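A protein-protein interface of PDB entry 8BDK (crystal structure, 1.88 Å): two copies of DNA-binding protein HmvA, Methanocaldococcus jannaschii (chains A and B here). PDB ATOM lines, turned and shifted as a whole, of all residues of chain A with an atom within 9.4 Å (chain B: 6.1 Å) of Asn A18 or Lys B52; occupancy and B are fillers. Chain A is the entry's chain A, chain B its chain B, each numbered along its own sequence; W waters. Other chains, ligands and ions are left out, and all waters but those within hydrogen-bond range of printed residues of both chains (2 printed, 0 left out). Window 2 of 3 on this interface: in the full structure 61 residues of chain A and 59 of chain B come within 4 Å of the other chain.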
ATOM      1  N   LYS A   8       6.066  16.566  -7.397  1.00  0.00           N
ATOM      2  CA  LYS A   8       6.532  17.841  -7.930  1.00  0.00           C
ATOM      3  C   LYS A   8       5.877  19.008  -7.202  1.00  0.00           C
ATOM      4  O   LYS A   8       6.518  20.039  -6.959  1.00  0.00           O
ATOM      5  CB  LYS A   8       6.259  17.929  -9.423  1.00  0.00           C
ATOM      6  CG  LYS A   8       6.806  19.216 -10.068  1.00  0.00           C
ATOM      7  CD  LYS A   8       6.445  19.238 -11.540  1.00  0.00           C
ATOM      8  CE  LYS A   8       7.021  20.462 -12.252  1.00  0.00           C
ATOM      9  NZ  LYS A   8       6.690  20.389 -13.690  1.00  0.00           N
ATOM     10  N   MET A  11       7.883  19.409  -4.080  1.00  0.00           N
ATOM     11  CA  MET A  11       9.156  20.021  -4.459  1.00  0.00           C
ATOM     12  C   MET A  11       9.020  21.526  -4.661  1.00  0.00           C
ATOM     13  O   MET A  11       9.874  22.299  -4.219  1.00  0.00           O
ATOM     14  CB  MET A  11       9.693  19.401  -5.750  1.00  0.00           C
ATOM     15  CG  MET A  11       9.994  17.949  -5.693  1.00  0.00           C
ATOM     16  SD  MET A  11      10.546  17.349  -7.320  1.00  0.00           S
ATOM     17  CE  MET A  11      12.248  17.857  -7.322  1.00  0.00           C
ATOM     18  N   LYS A  12       7.961  21.966  -5.342  1.00  0.00           N
ATOM     19  CA  LYS A  12       7.834  23.397  -5.592  1.00  0.00           C
ATOM     20  C   LYS A  12       7.404  24.163  -4.353  1.00  0.00           C
ATOM     21  O   LYS A  12       7.335  25.394  -4.401  1.00  0.00           O
ATOM     22  CB  LYS A  12       6.877  23.649  -6.755  1.00  0.00           C
ATOM     23  CG  LYS A  12       7.383  23.002  -8.028  1.00  0.00           C
ATOM     24  CD  LYS A  12       6.710  23.523  -9.264  1.00  0.00           C
ATOM     25  CE  LYS A  12       7.407  24.776  -9.778  1.00  0.00           C
ATOM     26  NZ  LYS A  12       6.972  25.072 -11.163  1.00  0.00           N
ATOM     27  N   THR A  15      11.157  25.307  -3.650  1.00  0.00           N
ATOM     28  CA  THR A  15      11.968  25.979  -4.653  1.00  0.00           C
ATOM     29  C   THR A  15      11.057  26.801  -5.548  1.00  0.00           C
ATOM     30  O   THR A  15       9.913  26.420  -5.810  1.00  0.00           O
ATOM     31  CB  THR A  15      12.790  24.981  -5.482  1.00  0.00           C
ATOM     32  OG1 THR A  15      13.645  25.691  -6.384  1.00  0.00           O
ATOM     33  CG2 THR A  15      11.891  24.004  -6.280  1.00  0.00           C
ATOM     34  N   ASP A  16      11.566  27.950  -5.985  1.00  0.00           N
ATOM     35  CA  ASP A  16      10.927  28.689  -7.059  1.00  0.00           C
ATOM     36  C   ASP A  16      11.332  28.159  -8.428  1.00  0.00           C
ATOM     37  O   ASP A  16      10.674  28.478  -9.419  1.00  0.00           O
ATOM     38  CB  ASP A  16      11.276  30.181  -6.955  1.00  0.00           C
ATOM     39  CG  ASP A  16      10.827  30.797  -5.635  1.00  0.00           C
ATOM     40  OD1 ASP A  16       9.950  30.195  -4.965  1.00  0.00           O
ATOM     41  OD2 ASP A  16      11.336  31.882  -5.269  1.00  0.00           O
ATOM     42  N   PHE A  17      12.382  27.339  -8.505  1.00  0.00           N
ATOM     43  CA  PHE A  17      12.924  26.933  -9.798  1.00  0.00           C
ATOM     44  C   PHE A  17      11.920  26.079 -10.564  1.00  0.00           C
ATOM     45  O   PHE A  17      11.066  25.410  -9.977  1.00  0.00           O
ATOM     46  CB  PHE A  17      14.243  26.155  -9.618  1.00  0.00           C
ATOM     47  CG  PHE A  17      15.449  27.032  -9.336  1.00  0.00           C
ATOM     48  CD1 PHE A  17      15.309  28.302  -8.778  1.00  0.00           C
ATOM     49  CD2 PHE A  17      16.721  26.588  -9.635  1.00  0.00           C
ATOM     50  CE1 PHE A  17      16.420  29.092  -8.521  1.00  0.00           C
ATOM     51  CE2 PHE A  17      17.837  27.381  -9.384  1.00  0.00           C
ATOM     52  CZ  PHE A  17      17.681  28.635  -8.826  1.00  0.00           C
ATOM     53  N   ASN A  18      12.017  26.114 -11.893  1.00  0.00           N
ATOM     54  CA  ASN A  18      11.364  25.091 -12.691  1.00  0.00           C
ATOM     55  C   ASN A  18      11.996  23.731 -12.372  1.00  0.00           C
ATOM     56  O   ASN A  18      13.120  23.645 -11.872  1.00  0.00           O
ATOM     57  CB  ASN A  18      11.476  25.406 -14.186  1.00  0.00           C
ATOM     58  CG  ASN A  18      10.585  26.563 -14.606  1.00  0.00           C
ATOM     59  OD1 ASN A  18       9.796  27.074 -13.810  1.00  0.00           O
ATOM     60  ND2 ASN A  18      10.703  26.977 -15.859  1.00  0.00           N
ATOM     61  N   ILE A  19      11.260  22.658 -12.651  1.00  0.00           N
ATOM     62  CA  ILE A  19      11.732  21.309 -12.348  1.00  0.00           C
ATOM     63  C   ILE A  19      11.416  20.401 -13.528  1.00  0.00           C
ATOM     64  O   ILE A  19      10.256  20.293 -13.940  1.00  0.00           O
ATOM     65  CB  ILE A  19      11.093  20.752 -11.063  1.00  0.00           C
ATOM     66  CG1 ILE A  19      11.227  21.775  -9.921  1.00  0.00           C
ATOM     67  CG2 ILE A  19      11.731  19.387 -10.719  1.00  0.00           C
ATOM     68  CD1 ILE A  19      10.542  21.392  -8.654  1.00  0.00           C
ATOM     69  N   SER A  20      12.435  19.729 -14.055  1.00  0.00           N
ATOM     70  CA  SER A  20      12.203  18.901 -15.231  1.00  0.00           C
ATOM     71  C   SER A  20      11.481  17.607 -14.861  1.00  0.00           C
ATOM     72  O   SER A  20      11.534  17.133 -13.719  1.00  0.00           O
ATOM     73  CB  SER A  20      13.516  18.565 -15.933  1.00  0.00           C
ATOM     74  OG  SER A  20      14.274  17.671 -15.147  1.00  0.00           O
ATOM     75  N   ALA A  21      10.796  17.030 -15.855  1.00  0.00           N
ATOM     76  CA  ALA A  21      10.131  15.747 -15.644  1.00  0.00           C
ATOM     77  C   ALA A  21      11.123  14.671 -15.223  1.00  0.00           C
ATOM     78  O   ALA A  21      10.816  13.837 -14.363  1.00  0.00           O
ATOM     79  CB  ALA A  21       9.390  15.319 -16.911  1.00  0.00           C
ATOM     80  N   ALA A  23      13.863  15.125 -13.496  1.00  0.00           N
ATOM     81  CA  ALA A  23      14.227  15.335 -12.094  1.00  0.00           C
ATOM     82  C   ALA A  23      13.153  14.795 -11.165  1.00  0.00           C
ATOM     83  O   ALA A  23      13.460  14.202 -10.125  1.00  0.00           O
ATOM     84  CB  ALA A  23      14.463  16.821 -11.811  1.00  0.00           C
ATOM     85  N   VAL A  24      11.887  15.021 -11.503  1.00  0.00           N
ATOM     86  CA  VAL A  24      10.806  14.492 -10.676  1.00  0.00           C
ATOM     87  C   VAL A  24      10.867  12.967 -10.628  1.00  0.00           C
ATOM     88  O   VAL A  24      10.734  12.359  -9.561  1.00  0.00           O
ATOM     89  CB  VAL A  24       9.452  15.000 -11.198  1.00  0.00           C
ATOM     90  CG1 VAL A  24       8.319  14.388 -10.405  1.00  0.00           C
ATOM     91  CG2 VAL A  24       9.405  16.520 -11.118  1.00  0.00           C
ATOM     92  N   ALA B  46      21.885  23.409  -9.438  1.00  0.00           N
ATOM     93  CA  ALA B  46      21.424  24.171 -10.584  1.00  0.00           C
ATOM     94  C   ALA B  46      22.059  25.560 -10.594  1.00  0.00           C
ATOM     95  O   ALA B  46      22.559  26.018 -11.630  1.00  0.00           O
ATOM     96  CB  ALA B  46      19.902  24.260 -10.565  1.00  0.00           C
ATOM     97  N   GLY B  50      24.536  27.948 -13.152  1.00  0.00           N
ATOM     98  CA  GLY B  50      23.909  29.110 -13.744  1.00  0.00           C
ATOM     99  C   GLY B  50      22.515  28.879 -14.265  1.00  0.00           C
ATOM    100  O   GLY B  50      22.070  29.611 -15.142  1.00  0.00           O
ATOM    101  N   ARG B  51      21.806  27.876 -13.756  1.00  0.00           N
ATOM    102  CA  ARG B  51      20.481  27.563 -14.269  1.00  0.00           C
ATOM    103  C   ARG B  51      19.400  27.934 -13.263  1.00  0.00           C
ATOM    104  O   ARG B  51      19.635  28.019 -12.055  1.00  0.00           O
ATOM    105  CB  ARG B  51      20.352  26.074 -14.625  1.00  0.00           C
ATOM    106  CG  ARG B  51      20.937  25.686 -15.971  1.00  0.00           C
ATOM    107  CD  ARG B  51      20.755  24.199 -16.250  1.00  0.00           C
ATOM    108  NE  ARG B  51      21.724  23.375 -15.527  1.00  0.00           N
ATOM    109  CZ  ARG B  51      21.438  22.633 -14.455  1.00  0.00           C
ATOM    110  NH1 ARG B  51      20.210  22.609 -13.963  1.00  0.00           N
ATOM    111  NH2 ARG B  51      22.386  21.916 -13.872  1.00  0.00           N
ATOM    112  N   LYS B  52      18.190  28.131 -13.786  1.00  0.00           N
ATOM    113  CA  LYS B  52      17.005  28.353 -12.972  1.00  0.00           C
ATOM    114  C   LYS B  52      15.999  27.221 -13.145  1.00  0.00           C
ATOM    115  O   LYS B  52      14.805  27.407 -12.891  1.00  0.00           O
ATOM    116  CB  LYS B  52      16.372  29.705 -13.310  1.00  0.00           C
ATOM    117  CG  LYS B  52      15.739  30.378 -12.119  1.00  0.00           C
ATOM    118  CD  LYS B  52      15.314  31.794 -12.432  1.00  0.00           C
ATOM    119  CE  LYS B  52      14.706  32.438 -11.200  1.00  0.00           C
ATOM    120  NZ  LYS B  52      14.414  33.879 -11.406  1.00  0.00           N
ATOM    121  N   THR B  53      16.475  26.056 -13.584  1.00  0.00           N
ATOM    122  CA  THR B  53      15.675  24.850 -13.752  1.00  0.00           C
ATOM    123  C   THR B  53      16.424  23.693 -13.111  1.00  0.00           C
ATOM    124  O   THR B  53      17.617  23.513 -13.367  1.00  0.00           O
ATOM    125  CB  THR B  53      15.418  24.541 -15.243  1.00  0.00           C
ATOM    126  OG1 THR B  53      14.671  25.605 -15.838  1.00  0.00           O
ATOM    127  CG2 THR B  53      14.635  23.241 -15.407  1.00  0.00           C
ATOM    128  N   ILE B  54      15.735  22.932 -12.266  1.00  0.00           N
ATOM    129  CA  ILE B  54      16.288  21.708 -11.704  1.00  0.00           C
ATOM    130  C   ILE B  54      16.168  20.619 -12.759  1.00  0.00           C
ATOM    131  O   ILE B  54      15.074  20.350 -13.273  1.00  0.00           O
ATOM    132  CB  ILE B  54      15.570  21.326 -10.400  1.00  0.00           C
ATOM    133  CG1 ILE B  54      15.963  22.304  -9.286  1.00  0.00           C
ATOM    134  CG2 ILE B  54      15.894  19.897  -9.931  1.00  0.00           C
ATOM    135  CD1 ILE B  54      15.282  21.980  -7.963  1.00  0.00           C
ATOM    136  N   LYS B  55      17.293  20.013 -13.110  1.00  0.00           N
ATOM    137  CA  LYS B  55      17.321  18.914 -14.061  1.00  0.00           C
ATOM    138  C   LYS B  55      17.854  17.660 -13.372  1.00  0.00           C
ATOM    139  O   LYS B  55      18.361  17.708 -12.251  1.00  0.00           O
ATOM    140  CB  LYS B  55      18.157  19.271 -15.291  1.00  0.00           C
ATOM    141  CG  LYS B  55      17.610  20.465 -16.074  1.00  0.00           C
HETATM  142  O   HOH W   1      12.603  25.254 -17.404  1.00  0.00           O
HETATM  143  O   HOH W   2      12.327  29.047 -13.537  1.00  0.00           O
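The backbone NH (N) of Asn A18 lies within hydrogen-bond range of the backbone carbonyl oxygen (O) of Lys B52 (3.2 Å). The backbone NH of Ser A20 sits at hydrogen-bond distance from the backbone carbonyl oxygen of Ile B54, at 2.8 Å. O of Asn A18 lies within hydrogen-bond range of N of Ile B54, 2.7 Å away.
The side-chain hydroxyl (OG1) of Thr A15 sits at hydrogen-bond distance from the backbone NH (N) of Phe A17 (3.0 Å). The side-chain hydroxyl (OG) of Ser A20 is in hydrogen-bond range of the backbone NH (N) of Ala A23 (3.1 Å). O of Ala B46 sits at hydrogen-bond distance from N of Arg B51, at 2.9 Å. The backbone carbonyl oxygen (O) of Thr B53 lies within hydrogen-bond range of the guanidinium group (NH1) of Arg B51, 2.8 Å away.
Water W1 lies within hydrogen-bond range of OG1 of Thr B53 (2.6 Å) and ND2 of Asn A18 (3.0 Å). Water W2 bridges O of Lys B52 and OD1 of Asn A18.
Of the printed residues of chain B, Asn A18 touches Lys B52 (3.2 Å), Thr B53 (3.4 Å) and Ile B54 (2.7 Å). Of chain A, only Phe A17 (3.5 Å) and Asn A18 (3.2 Å) come within 4 Å of Lys B52. Ile B54 touches four residues of chain A. Of the printed residues of chain B, Ile A19 touches Ile B54. Of the printed residues of chain B, Ser A20 touches Ile B54 (2.8 Å) and Lys B55 (3.5 Å). Asp A16 touches none of the printed residues of chain B. The nearest printed residue of chain A that does not touch Lys B55 is Asn A18 (5.7 Å).
Hydrophobic or aromatic side chains of chain A within 4 Å of the printed part of chain B: Phe A17 and Ala A23. Of the 7 printed residues of chain B, 6 touch a printed residue of chain A. Printed residues of chain B that touch a printed residue of chain A: Ala B46, Arg B51, Lys B52, Thr B53, Ile B54 and Lys B55. Among the printed residues, 12 pairs touch across the chains. Among the printed residues, no Asp or Glu carboxylate lies within 4 Å of a Lys or Arg side-chain nitrogen of the other chain.
No position is printed for both chains.
Among the printed residues, merely in contact across the chains: Phe A17 with Ala B46, Phe A17 with Arg B51, Phe A17 with Lys B52, Phe A17 with Thr B53, Asn A18 with Thr B53, Ile A19 with Ile B54, Ser A20 with Lys B55, Ala A23 with Ile B54 and Ala A23 with Lys B55.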
